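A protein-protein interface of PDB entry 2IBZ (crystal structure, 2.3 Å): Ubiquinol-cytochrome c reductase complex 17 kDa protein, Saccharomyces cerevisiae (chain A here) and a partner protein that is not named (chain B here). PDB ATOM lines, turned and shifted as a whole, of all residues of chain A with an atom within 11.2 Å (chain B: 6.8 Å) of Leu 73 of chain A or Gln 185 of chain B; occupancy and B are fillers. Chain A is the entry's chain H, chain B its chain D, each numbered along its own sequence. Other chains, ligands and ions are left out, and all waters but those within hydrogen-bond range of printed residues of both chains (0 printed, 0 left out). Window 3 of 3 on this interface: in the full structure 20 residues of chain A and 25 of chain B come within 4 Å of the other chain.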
ATOM      1  N   VAL A   1      33.759  16.702 -20.221  1.00  0.00           N
ATOM      2  CA  VAL A   1      33.594  17.553 -21.441  1.00  0.00           C
ATOM      3  C   VAL A   1      32.222  18.233 -21.385  1.00  0.00           C
ATOM      4  O   VAL A   1      31.549  18.201 -20.349  1.00  0.00           O
ATOM      5  CB  VAL A   1      33.696  16.704 -22.748  1.00  0.00           C
ATOM      6  CG1 VAL A   1      34.120  17.583 -23.919  1.00  0.00           C
ATOM      7  CG2 VAL A   1      34.674  15.543 -22.571  1.00  0.00           C
ATOM      8  N   THR A   2      31.828  18.872 -22.486  1.00  0.00           N
ATOM      9  CA  THR A   2      30.536  19.552 -22.578  1.00  0.00           C
ATOM     10  C   THR A   2      29.495  18.596 -23.189  1.00  0.00           C
ATOM     11  O   THR A   2      29.814  17.822 -24.105  1.00  0.00           O
ATOM     12  CB  THR A   2      30.651  20.845 -23.434  1.00  0.00           C
ATOM     13  OG1 THR A   2      29.384  21.515 -23.482  1.00  0.00           O
ATOM     14  CG2 THR A   2      31.111  20.519 -24.856  1.00  0.00           C
ATOM     15  N   ASP A   3      28.262  18.640 -22.673  1.00  0.00           N
ATOM     16  CA  ASP A   3      27.192  17.771 -23.170  1.00  0.00           C
ATOM     17  C   ASP A   3      27.024  17.830 -24.687  1.00  0.00           C
ATOM     18  O   ASP A   3      26.844  18.904 -25.261  1.00  0.00           O
ATOM     19  CB  ASP A   3      25.854  18.077 -22.494  1.00  0.00           C
ATOM     20  CG  ASP A   3      24.733  17.181 -23.008  1.00  0.00           C
ATOM     21  OD1 ASP A   3      24.920  15.944 -23.000  1.00  0.00           O
ATOM     22  OD2 ASP A   3      23.685  17.710 -23.447  1.00  0.00           O
ATOM     23  N   GLN A   4      27.037  16.653 -25.309  1.00  0.00           N
ATOM     24  CA  GLN A   4      26.930  16.501 -26.755  1.00  0.00           C
ATOM     25  C   GLN A   4      25.612  16.976 -27.364  1.00  0.00           C
ATOM     26  O   GLN A   4      25.586  17.474 -28.490  1.00  0.00           O
ATOM     27  CB  GLN A   4      27.186  15.043 -27.140  1.00  0.00           C
ATOM     28  CG  GLN A   4      28.564  14.497 -26.756  1.00  0.00           C
ATOM     29  CD  GLN A   4      28.635  13.900 -25.353  1.00  0.00           C
ATOM     30  OE1 GLN A   4      29.490  13.058 -25.073  1.00  0.00           O
ATOM     31  NE2 GLN A   4      27.744  14.332 -24.469  1.00  0.00           N
ATOM     32  N   LEU A   5      24.519  16.807 -26.628  1.00  0.00           N
ATOM     33  CA  LEU A   5      23.206  17.226 -27.099  1.00  0.00           C
ATOM     34  C   LEU A   5      23.090  18.753 -27.054  1.00  0.00           C
ATOM     35  O   LEU A   5      22.664  19.376 -28.032  1.00  0.00           O
ATOM     36  CB  LEU A   5      22.105  16.566 -26.259  1.00  0.00           C
ATOM     37  CG  LEU A   5      20.640  16.795 -26.640  1.00  0.00           C
ATOM     38  CD1 LEU A   5      20.364  16.323 -28.053  1.00  0.00           C
ATOM     39  CD2 LEU A   5      19.759  16.057 -25.668  1.00  0.00           C
ATOM     40  N   GLU A   6      23.477  19.348 -25.925  1.00  0.00           N
ATOM     41  CA  GLU A   6      23.432  20.801 -25.764  1.00  0.00           C
ATOM     42  C   GLU A   6      24.271  21.480 -26.832  1.00  0.00           C
ATOM     43  O   GLU A   6      23.932  22.567 -27.298  1.00  0.00           O
ATOM     44  CB  GLU A   6      23.947  21.224 -24.388  1.00  0.00           C
ATOM     45  CG  GLU A   6      22.943  21.063 -23.272  1.00  0.00           C
ATOM     46  CD  GLU A   6      23.044  22.176 -22.247  1.00  0.00           C
ATOM     47  OE1 GLU A   6      23.757  21.994 -21.233  1.00  0.00           O
ATOM     48  OE2 GLU A   6      22.414  23.239 -22.464  1.00  0.00           O
ATOM     49  N   ASP A   7      25.369  20.827 -27.201  1.00  0.00           N
ATOM     50  CA  ASP A   7      26.274  21.326 -28.224  1.00  0.00           C
ATOM     51  C   ASP A   7      25.547  21.405 -29.566  1.00  0.00           C
ATOM     52  O   ASP A   7      25.467  22.475 -30.165  1.00  0.00           O
ATOM     53  CB  ASP A   7      27.488  20.401 -28.333  1.00  0.00           C
ATOM     54  CG  ASP A   7      28.496  20.874 -29.364  1.00  0.00           C
ATOM     55  OD1 ASP A   7      29.433  21.610 -28.975  1.00  0.00           O
ATOM     56  OD2 ASP A   7      28.358  20.505 -30.556  1.00  0.00           O
ATOM     57  N   LEU A   8      25.007  20.272 -30.020  1.00  0.00           N
ATOM     58  CA  LEU A   8      24.275  20.202 -31.287  1.00  0.00           C
ATOM     59  C   LEU A   8      23.037  21.104 -31.320  1.00  0.00           C
ATOM     60  O   LEU A   8      22.662  21.612 -32.379  1.00  0.00           O
ATOM     61  CB  LEU A   8      23.899  18.751 -31.615  1.00  0.00           C
ATOM     62  CG  LEU A   8      24.998  17.866 -32.207  1.00  0.00           C
ATOM     63  CD1 LEU A   8      24.492  16.448 -32.381  1.00  0.00           C
ATOM     64  CD2 LEU A   8      25.435  18.427 -33.543  1.00  0.00           C
ATOM     65  N   THR A  65      19.070  17.241 -34.529  1.00  0.00           N
ATOM     66  CA  THR A  65      19.970  16.619 -33.566  1.00  0.00           C
ATOM     67  C   THR A  65      19.844  15.100 -33.436  1.00  0.00           C
ATOM     68  O   THR A  65      20.847  14.398 -33.297  1.00  0.00           O
ATOM     69  CB  THR A  65      19.815  17.248 -32.170  1.00  0.00           C
ATOM     70  OG1 THR A  65      18.494  17.013 -31.679  1.00  0.00           O
ATOM     71  CG2 THR A  65      20.062  18.743 -32.232  1.00  0.00           C
ATOM     72  N   ALA A  66      18.616  14.595 -33.520  1.00  0.00           N
ATOM     73  CA  ALA A  66      18.347  13.164 -33.383  1.00  0.00           C
ATOM     74  C   ALA A  66      19.152  12.199 -34.259  1.00  0.00           C
ATOM     75  O   ALA A  66      19.600  11.155 -33.780  1.00  0.00           O
ATOM     76  CB  ALA A  66      16.853  12.892 -33.526  1.00  0.00           C
ATOM     77  N   PRO A  67      19.315  12.503 -35.553  1.00  0.00           N
ATOM     78  CA  PRO A  67      20.083  11.584 -36.403  1.00  0.00           C
ATOM     79  C   PRO A  67      21.609  11.660 -36.263  1.00  0.00           C
ATOM     80  O   PRO A  67      22.331  10.830 -36.818  1.00  0.00           O
ATOM     81  CB  PRO A  67      19.634  11.979 -37.812  1.00  0.00           C
ATOM     82  CG  PRO A  67      19.383  13.434 -37.680  1.00  0.00           C
ATOM     83  CD  PRO A  67      18.646  13.534 -36.366  1.00  0.00           C
ATOM     84  N   ARG A  68      22.088  12.609 -35.465  1.00  0.00           N
ATOM     85  CA  ARG A  68      23.522  12.821 -35.289  1.00  0.00           C
ATOM     86  C   ARG A  68      24.066  12.593 -33.890  1.00  0.00           C
ATOM     87  O   ARG A  68      25.225  12.208 -33.736  1.00  0.00           O
ATOM     88  CB  ARG A  68      23.887  14.249 -35.720  1.00  0.00           C
ATOM     89  CG  ARG A  68      23.940  14.481 -37.218  1.00  0.00           C
ATOM     90  CD  ARG A  68      24.304  15.929 -37.543  1.00  0.00           C
ATOM     91  NE  ARG A  68      23.116  16.756 -37.727  1.00  0.00           N
ATOM     92  CZ  ARG A  68      22.608  17.079 -38.915  1.00  0.00           C
ATOM     93  NH1 ARG A  68      21.513  17.827 -38.988  1.00  0.00           N
ATOM     94  NH2 ARG A  68      23.201  16.669 -40.033  1.00  0.00           N
ATOM     95  N   LEU A  69      23.243  12.822 -32.874  1.00  0.00           N
ATOM     96  CA  LEU A  69      23.680  12.688 -31.489  1.00  0.00           C
ATOM     97  C   LEU A  69      24.442  11.415 -31.096  1.00  0.00           C
ATOM     98  O   LEU A  69      25.456  11.492 -30.392  1.00  0.00           O
ATOM     99  CB  LEU A  69      22.507  12.905 -30.533  1.00  0.00           C
ATOM    100  CG  LEU A  69      22.881  12.800 -29.054  1.00  0.00           C
ATOM    101  CD1 LEU A  69      23.971  13.817 -28.731  1.00  0.00           C
ATOM    102  CD2 LEU A  69      21.662  13.013 -28.179  1.00  0.00           C
ATOM    103  N   PHE A  70      23.976  10.256 -31.555  1.00  0.00           N
ATOM    104  CA  PHE A  70      24.625   9.003 -31.189  1.00  0.00           C
ATOM    105  C   PHE A  70      25.999   8.713 -31.804  1.00  0.00           C
ATOM    106  O   PHE A  70      26.786   7.948 -31.238  1.00  0.00           O
ATOM    107  CB  PHE A  70      23.645   7.827 -31.324  1.00  0.00           C
ATOM    108  CG  PHE A  70      22.621   7.771 -30.214  1.00  0.00           C
ATOM    109  CD1 PHE A  70      22.150   8.938 -29.622  1.00  0.00           C
ATOM    110  CD2 PHE A  70      22.152   6.557 -29.739  1.00  0.00           C
ATOM    111  CE1 PHE A  70      21.231   8.897 -28.574  1.00  0.00           C
ATOM    112  CE2 PHE A  70      21.232   6.506 -28.693  1.00  0.00           C
ATOM    113  CZ  PHE A  70      20.770   7.680 -28.108  1.00  0.00           C
ATOM    114  N   ASP A  71      26.306   9.329 -32.941  1.00  0.00           N
ATOM    115  CA  ASP A  71      27.624   9.139 -33.540  1.00  0.00           C
ATOM    116  C   ASP A  71      28.673   9.821 -32.656  1.00  0.00           C
ATOM    117  O   ASP A  71      29.864   9.535 -32.754  1.00  0.00           O
ATOM    118  CB  ASP A  71      27.680   9.711 -34.955  1.00  0.00           C
ATOM    119  CG  ASP A  71      27.029   8.802 -35.974  1.00  0.00           C
ATOM    120  OD1 ASP A  71      26.222   9.307 -36.782  1.00  0.00           O
ATOM    121  OD2 ASP A  71      27.324   7.582 -35.970  1.00  0.00           O
ATOM    122  N   LYS A  72      28.214  10.713 -31.783  1.00  0.00           N
ATOM    123  CA  LYS A  72      29.104  11.418 -30.876  1.00  0.00           C
ATOM    124  C   LYS A  72      29.159  10.766 -29.497  1.00  0.00           C
ATOM    125  O   LYS A  72      30.016  11.095 -28.684  1.00  0.00           O
ATOM    126  CB  LYS A  72      28.703  12.895 -30.766  1.00  0.00           C
ATOM    127  CG  LYS A  72      28.926  13.687 -32.056  1.00  0.00           C
ATOM    128  CD  LYS A  72      30.357  13.483 -32.589  1.00  0.00           C
ATOM    129  CE  LYS A  72      30.603  14.236 -33.891  1.00  0.00           C
ATOM    130  NZ  LYS A  72      30.457  15.718 -33.726  1.00  0.00           N
ATOM    131  N   LEU A  73      28.244   9.839 -29.240  1.00  0.00           N
ATOM    132  CA  LEU A  73      28.200   9.140 -27.963  1.00  0.00           C
ATOM    133  C   LEU A  73      28.899   7.793 -28.053  1.00  0.00           C
ATOM    134  O   LEU A  73      29.199   7.301 -29.142  1.00  0.00           O
ATOM    135  CB  LEU A  73      26.756   8.938 -27.500  1.00  0.00           C
ATOM    136  CG  LEU A  73      25.929  10.173 -27.141  1.00  0.00           C
ATOM    137  CD1 LEU A  73      24.542   9.744 -26.688  1.00  0.00           C
ATOM    138  CD2 LEU A  73      26.616  10.956 -26.039  1.00  0.00           C
ATOM    139  N   LYS A  74      29.179   7.216 -26.892  1.00  0.00           N
ATOM    140  CA  LYS A  74      29.829   5.920 -26.820  1.00  0.00           C
ATOM    141  C   LYS A  74      28.779   4.864 -26.469  1.00  0.00           C
ATOM    142  O   LYS A  74      27.952   5.123 -25.568  1.00  0.00           O
ATOM    143  CB  LYS A  74      30.966   5.961 -25.781  1.00  0.00           C
ATOM    144  CG  LYS A  74      31.583   4.603 -25.409  1.00  0.00           C
ATOM    145  CD  LYS A  74      32.203   3.865 -26.608  1.00  0.00           C
ATOM    146  CE  LYS A  74      32.789   2.495 -26.205  1.00  0.00           C
ATOM    147  NZ  LYS A  74      31.787   1.513 -25.651  1.00  0.00           N
ATOM    148  OXT LYS A  74      28.783   3.801 -27.126  1.00  0.00           O
ATOM    149  N   SER B  28      26.925  -0.581 -22.596  1.00  0.00           N
ATOM    150  CA  SER B  28      25.950   0.455 -22.283  1.00  0.00           C
ATOM    151  C   SER B  28      24.992  -0.060 -21.200  1.00  0.00           C
ATOM    152  O   SER B  28      24.608   0.687 -20.290  1.00  0.00           O
ATOM    153  CB  SER B  28      25.183   0.851 -23.533  1.00  0.00           C
ATOM    154  OG  SER B  28      24.497   2.066 -23.317  1.00  0.00           O
ATOM    155  N   ARG B  31      26.891   0.223 -17.895  1.00  0.00           N
ATOM    156  CA  ARG B  31      26.915   1.610 -17.442  1.00  0.00           C
ATOM    157  C   ARG B  31      25.539   2.066 -16.956  1.00  0.00           C
ATOM    158  O   ARG B  31      25.436   2.723 -15.914  1.00  0.00           O
ATOM    159  CB  ARG B  31      27.384   2.525 -18.573  1.00  0.00           C
ATOM    160  CG  ARG B  31      28.900   2.630 -18.728  1.00  0.00           C
ATOM    161  CD  ARG B  31      29.265   3.529 -19.898  1.00  0.00           C
ATOM    162  NE  ARG B  31      29.624   2.766 -21.087  1.00  0.00           N
ATOM    163  CZ  ARG B  31      29.186   3.030 -22.308  1.00  0.00           C
ATOM    164  NH1 ARG B  31      29.577   2.284 -23.333  1.00  0.00           N
ATOM    165  NH2 ARG B  31      28.327   4.011 -22.506  1.00  0.00           N
ATOM    166  N   VAL B  35      24.145   4.155 -13.426  1.00  0.00           N
ATOM    167  CA  VAL B  35      23.339   5.366 -13.409  1.00  0.00           C
ATOM    168  C   VAL B  35      22.071   5.077 -12.624  1.00  0.00           C
ATOM    169  O   VAL B  35      21.625   5.904 -11.827  1.00  0.00           O
ATOM    170  CB  VAL B  35      22.984   5.825 -14.831  1.00  0.00           C
ATOM    171  CG1 VAL B  35      22.048   7.034 -14.786  1.00  0.00           C
ATOM    172  CG2 VAL B  35      24.252   6.160 -15.607  1.00  0.00           C
ATOM    173  N   PHE B 131      14.526   8.620 -23.243  1.00  0.00           N
ATOM    174  CA  PHE B 131      15.714   9.409 -23.443  1.00  0.00           C
ATOM    175  C   PHE B 131      15.356  10.893 -23.549  1.00  0.00           C
ATOM    176  O   PHE B 131      15.869  11.724 -22.794  1.00  0.00           O
ATOM    177  CB  PHE B 131      16.456   8.961 -24.697  1.00  0.00           C
ATOM    178  CG  PHE B 131      17.727   9.722 -24.932  1.00  0.00           C
ATOM    179  CD1 PHE B 131      18.908   9.333 -24.309  1.00  0.00           C
ATOM    180  CD2 PHE B 131      17.739  10.851 -25.737  1.00  0.00           C
ATOM    181  CE1 PHE B 131      20.078  10.061 -24.487  1.00  0.00           C
ATOM    182  CE2 PHE B 131      18.899  11.580 -25.920  1.00  0.00           C
ATOM    183  CZ  PHE B 131      20.078  11.184 -25.290  1.00  0.00           C
ATOM    184  N   THR B 135      16.460  14.240 -21.123  1.00  0.00           N
ATOM    185  CA  THR B 135      17.316  15.276 -21.667  1.00  0.00           C
ATOM    186  C   THR B 135      16.509  16.470 -22.170  1.00  0.00           C
ATOM    187  O   THR B 135      17.059  17.390 -22.782  1.00  0.00           O
ATOM    188  CB  THR B 135      18.106  14.722 -22.853  1.00  0.00           C
ATOM    189  OG1 THR B 135      17.190  14.218 -23.832  1.00  0.00           O
ATOM    190  CG2 THR B 135      19.024  13.599 -22.410  1.00  0.00           C
ATOM    191  N   LEU B 168      19.602  14.468 -14.101  1.00  0.00           N
ATOM    192  CA  LEU B 168      20.872  14.179 -14.745  1.00  0.00           C
ATOM    193  C   LEU B 168      21.610  15.477 -15.012  1.00  0.00           C
ATOM    194  O   LEU B 168      21.044  16.418 -15.577  1.00  0.00           O
ATOM    195  CB  LEU B 168      20.669  13.425 -16.064  1.00  0.00           C
ATOM    196  CG  LEU B 168      20.105  12.006 -15.983  1.00  0.00           C
ATOM    197  CD1 LEU B 168      19.992  11.424 -17.384  1.00  0.00           C
ATOM    198  CD2 LEU B 168      20.998  11.140 -15.115  1.00  0.00           C
ATOM    199  N   TYR B 175      32.018   6.980 -14.392  1.00  0.00           N
ATOM    200  CA  TYR B 175      31.979   5.703 -15.096  1.00  0.00           C
ATOM    201  C   TYR B 175      33.218   4.869 -14.870  1.00  0.00           C
ATOM    202  O   TYR B 175      34.345   5.320 -15.081  1.00  0.00           O
ATOM    203  CB  TYR B 175      31.741   5.893 -16.593  1.00  0.00           C
ATOM    204  CG  TYR B 175      30.286   6.076 -16.967  1.00  0.00           C
ATOM    205  CD1 TYR B 175      29.924   6.851 -18.071  1.00  0.00           C
ATOM    206  CD2 TYR B 175      29.267   5.474 -16.215  1.00  0.00           C
ATOM    207  CE1 TYR B 175      28.592   7.025 -18.416  1.00  0.00           C
ATOM    208  CE2 TYR B 175      27.930   5.640 -16.554  1.00  0.00           C
ATOM    209  CZ  TYR B 175      27.599   6.418 -17.653  1.00  0.00           C
ATOM    210  OH  TYR B 175      26.281   6.605 -17.990  1.00  0.00           O
ATOM    211  N   THR B 179      34.457   6.346 -19.493  1.00  0.00           N
ATOM    212  CA  THR B 179      33.614   7.113 -20.416  1.00  0.00           C
ATOM    213  C   THR B 179      33.166   8.449 -19.812  1.00  0.00           C
ATOM    214  O   THR B 179      32.847   8.530 -18.618  1.00  0.00           O
ATOM    215  CB  THR B 179      32.376   6.267 -20.847  1.00  0.00           C
ATOM    216  OG1 THR B 179      32.826   5.077 -21.511  1.00  0.00           O
ATOM    217  CG2 THR B 179      31.457   7.052 -21.786  1.00  0.00           C
ATOM    218  N   PRO B 180      33.206   9.531 -20.616  1.00  0.00           N
ATOM    219  CA  PRO B 180      32.793  10.858 -20.139  1.00  0.00           C
ATOM    220  C   PRO B 180      31.300  10.818 -19.792  1.00  0.00           C
ATOM    221  O   PRO B 180      30.443  10.639 -20.667  1.00  0.00           O
ATOM    222  CB  PRO B 180      33.048  11.768 -21.353  1.00  0.00           C
ATOM    223  CG  PRO B 180      34.088  11.034 -22.152  1.00  0.00           C
ATOM    224  CD  PRO B 180      33.679   9.590 -22.013  1.00  0.00           C
ATOM    225  N   ALA B 181      30.997  11.002 -18.516  1.00  0.00           N
ATOM    226  CA  ALA B 181      29.631  10.963 -18.050  1.00  0.00           C
ATOM    227  C   ALA B 181      28.779  12.197 -18.312  1.00  0.00           C
ATOM    228  O   ALA B 181      28.276  12.814 -17.371  1.00  0.00           O
ATOM    229  CB  ALA B 181      29.598  10.596 -16.580  1.00  0.00           C
ATOM    230  N   THR B 182      28.596  12.552 -19.582  1.00  0.00           N
ATOM    231  CA  THR B 182      27.739  13.690 -19.924  1.00  0.00           C
ATOM    232  C   THR B 182      26.273  13.287 -19.692  1.00  0.00           C
ATOM    233  O   THR B 182      25.961  12.092 -19.618  1.00  0.00           O
ATOM    234  CB  THR B 182      27.914  14.127 -21.379  1.00  0.00           C
ATOM    235  OG1 THR B 182      27.630  13.026 -22.248  1.00  0.00           O
ATOM    236  CG2 THR B 182      29.337  14.617 -21.624  1.00  0.00           C
ATOM    237  N   THR B 183      25.375  14.267 -19.584  1.00  0.00           N
ATOM    238  CA  THR B 183      23.969  13.956 -19.322  1.00  0.00           C
ATOM    239  C   THR B 183      23.323  13.113 -20.414  1.00  0.00           C
ATOM    240  O   THR B 183      22.589  12.171 -20.114  1.00  0.00           O
ATOM    241  CB  THR B 183      23.092  15.213 -19.075  1.00  0.00           C
ATOM    242  OG1 THR B 183      22.524  15.659 -20.312  1.00  0.00           O
ATOM    243  CG2 THR B 183      23.904  16.334 -18.453  1.00  0.00           C
ATOM    244  N   SER B 184      23.623  13.435 -21.668  1.00  0.00           N
ATOM    245  CA  SER B 184      23.053  12.701 -22.789  1.00  0.00           C
ATOM    246  C   SER B 184      23.643  11.297 -22.867  1.00  0.00           C
ATOM    247  O   SER B 184      22.996  10.370 -23.355  1.00  0.00           O
ATOM    248  CB  SER B 184      23.255  13.456 -24.109  1.00  0.00           C
ATOM    249  OG  SER B 184      24.568  13.280 -24.609  1.00  0.00           O
ATOM    250  N   GLN B 185      24.867  11.142 -22.375  1.00  0.00           N
ATOM    251  CA  GLN B 185      25.535   9.841 -22.369  1.00  0.00           C
ATOM    252  C   GLN B 185      24.911   8.955 -21.301  1.00  0.00           C
ATOM    253  O   GLN B 185      24.694   7.767 -21.524  1.00  0.00           O
ATOM    254  CB  GLN B 185      27.028  10.011 -22.089  1.00  0.00           C
ATOM    255  CG  GLN B 185      27.770   8.725 -21.856  1.00  0.00           C
ATOM    256  CD  GLN B 185      28.055   7.952 -23.121  1.00  0.00           C
ATOM    257  OE1 GLN B 185      28.460   8.515 -24.144  1.00  0.00           O
ATOM    258  NE2 GLN B 185      27.888   6.643 -23.048  1.00  0.00           N
ATOM    259  N   MET B 186      24.650   9.537 -20.133  1.00  0.00           N
ATOM    260  CA  MET B 186      24.049   8.801 -19.035  1.00  0.00           C
ATOM    261  C   MET B 186      22.612   8.428 -19.372  1.00  0.00           C
ATOM    262  O   MET B 186      22.160   7.337 -19.043  1.00  0.00           O
ATOM    263  CB  MET B 186      24.085   9.622 -17.751  1.00  0.00           C
ATOM    264  CG  MET B 186      25.486   9.817 -17.195  1.00  0.00           C
ATOM    265  SD  MET B 186      25.430  10.673 -15.640  1.00  0.00           S
ATOM    266  CE  MET B 186      24.982  12.318 -16.216  1.00  0.00           C
ATOM    267  N   ALA B 187      21.904   9.339 -20.033  1.00  0.00           N
ATOM    268  CA  ALA B 187      20.532   9.097 -20.432  1.00  0.00           C
ATOM    269  C   ALA B 187      20.528   7.929 -21.408  1.00  0.00           C
ATOM    270  O   ALA B 187      19.757   6.990 -21.253  1.00  0.00           O
ATOM    271  CB  ALA B 187      19.958  10.331 -21.085  1.00  0.00           C
ATOM    272  N   LYS B 188      21.440   7.970 -22.375  1.00  0.00           N
ATOM    273  CA  LYS B 188      21.562   6.918 -23.376  1.00  0.00           C
ATOM    274  C   LYS B 188      21.803   5.563 -22.714  1.00  0.00           C
ATOM    275  O   LYS B 188      21.201   4.571 -23.104  1.00  0.00           O
ATOM    276  CB  LYS B 188      22.695   7.262 -24.351  1.00  0.00           C
ATOM    277  CG  LYS B 188      22.864   6.338 -25.555  1.00  0.00           C
ATOM    278  CD  LYS B 188      23.884   5.235 -25.297  1.00  0.00           C
ATOM    279  CE  LYS B 188      24.476   4.693 -26.589  1.00  0.00           C
ATOM    280  NZ  LYS B 188      25.271   3.446 -26.346  1.00  0.00           N
ATOM    281  N   ASP B 189      22.628   5.544 -21.671  1.00  0.00           N
ATOM    282  CA  ASP B 189      22.952   4.310 -20.965  1.00  0.00           C
ATOM    283  C   ASP B 189      21.823   3.725 -20.105  1.00  0.00           C
ATOM    284  O   ASP B 189      21.569   2.530 -20.198  1.00  0.00           O
ATOM    285  CB  ASP B 189      24.225   4.480 -20.104  1.00  0.00           C
ATOM    286  CG  ASP B 189      25.497   4.719 -20.936  1.00  0.00           C
ATOM    287  OD1 ASP B 189      25.557   4.330 -22.124  1.00  0.00           O
ATOM    288  OD2 ASP B 189      26.457   5.299 -20.380  1.00  0.00           O
ATOM    289  N   VAL B 190      21.193   4.519 -19.229  1.00  0.00           N
ATOM    290  CA  VAL B 190      20.114   3.967 -18.396  1.00  0.00           C
ATOM    291  C   VAL B 190      18.992   3.470 -19.276  1.00  0.00           C
ATOM    292  O   VAL B 190      18.375   2.446 -19.002  1.00  0.00           O
ATOM    293  CB  VAL B 190      19.431   4.978 -17.449  1.00  0.00           C
ATOM    294  CG1 VAL B 190      19.893   4.788 -16.060  1.00  0.00           C
ATOM    295  CG2 VAL B 190      19.568   6.374 -17.939  1.00  0.00           C
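No residue of chain A comes within 4 Å of Pro 180 of chain B.
No residue of chain A comes within 4 Å of Ala 181 of chain B.
Of chain A, only Asp 3 (3.9 Å) and Gln 4 (2.6 Å) come within 4 Å of Thr 182 of chain B.
Thr 183 of chain B touches just one residue of chain A: Asp 3.
Of chain A, only Asp 3, Gln 4, Leu 5 and Leu 73 come within 4 Å of Ser 184 of chain B.
Of chain A, only Phe 70 (3.5 Å), Leu 73 (3.9 Å) and Lys 74 (3.3 Å) come within 4 Å of Lys 188 of chain B.
Of the printed residues of chain A, Thr 135 of chain B touches Leu 5.
Printed residues of chain A within 4 Å of Arg 31 of chain B: Lys 74 (3.3 Å).
Printed residues of chain B within 4 Å of Leu 69 of chain A: Phe 131.
Of the printed residues of chain B, Leu 5 of chain A touches Thr 135 and Ser 184.
Tyr 175 of chain B touches none of the printed residues of chain A.
Ala 66 of chain A touches none of the printed residues of chain B.
The nearest residue of chain B that does not touch Leu 73 of chain A is Thr 182 of chain B (4.4 Å).
Among the printed residues, merely in contact across the chains: Leu 73 of chain A with Ser 184 of chain B (3.4 Å), Leu 5 of chain A with Thr 135 of chain B (3.5 Å), Phe 70 of chain A with Lys 188 of chain B (3.5 Å), Leu 73 of chain A with Gln 185 of chain B (3.6 Å), Asp 3 of chain A with Thr 183 of chain B (3.6 Å), Leu 69 of chain A with Phe 131 of chain B (3.8 Å), Asp 3 of chain A with Thr 182 of chain B (3.9 Å), Leu 73 of chain A with Lys 188 of chain B (3.9 Å) and Leu 5 of chain A with Ser 184 of chain B (3.95 Å).
The guanidinium group (NH2) of Arg 31 of chain B lies within salt-bridge range of the chain-end carboxylate (O) of Lys 74 of chain A.
OG1 of Thr 182 of chain B lies within hydrogen-bond range of NE2 of Gln 4 of chain A (2.6 Å).
N of Ser 184 of chain B sits at hydrogen-bond distance from OD1 of Asp 3 of chain A (3.1 Å).
The side-chain hydroxyl of Ser 184 of chain B lies within hydrogen-bond range of the side-chain amide nitrogen of Gln 4 of chain A.
The side-chain amide nitrogen of Gln 185 of chain B sits at hydrogen-bond distance from the chain-end carboxylate of Lys 74 of chain A (2.9 Å).
The side-chain amino group (NZ) of Lys 188 of chain B is in salt-bridge range of the chain-end carboxylate (O) of Lys 74 of chain A, 3.3 Å away.
OG of Ser 28 of chain B sits at hydrogen-bond distance from NZ of Lys 188 of chain B (3.4 Å).
The guanidinium group (NH2) of Arg 31 of chain B sits close to the side-chain amide nitrogen (NE2) of Gln 185 of chain B (2.7 Å).
The backbone NH (N) of Gln 185 of chain B sits close to the side-chain hydroxyl (OG1) of Thr 182 of chain B (3.3 Å).
NE2 of Gln 185 of chain B is in hydrogen-bond range of OD2 of Asp 189 of chain B (3.3 Å).
OD2 of Asp 3 of chain A sits close to N of Leu 5 of chain A (3.4 Å).
The side-chain carboxylate (OD2) of Asp 3 of chain A lies within hydrogen-bond range of the backbone NH (N) of Glu 6 of chain A, 3.0 Å away.
Of the 19 printed residues of chain B, 8 touch a printed residue of chain A.
Hydrophobic or aromatic side chains of chain B that line the printed part of chain A: Phe 131.
Of the 18 printed residues of chain A, 7 touch a printed residue of chain B.
Among the printed residues, no Asp or Glu carboxylate lies within 4 Å of a Lys or Arg side-chain nitrogen of the other chain.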
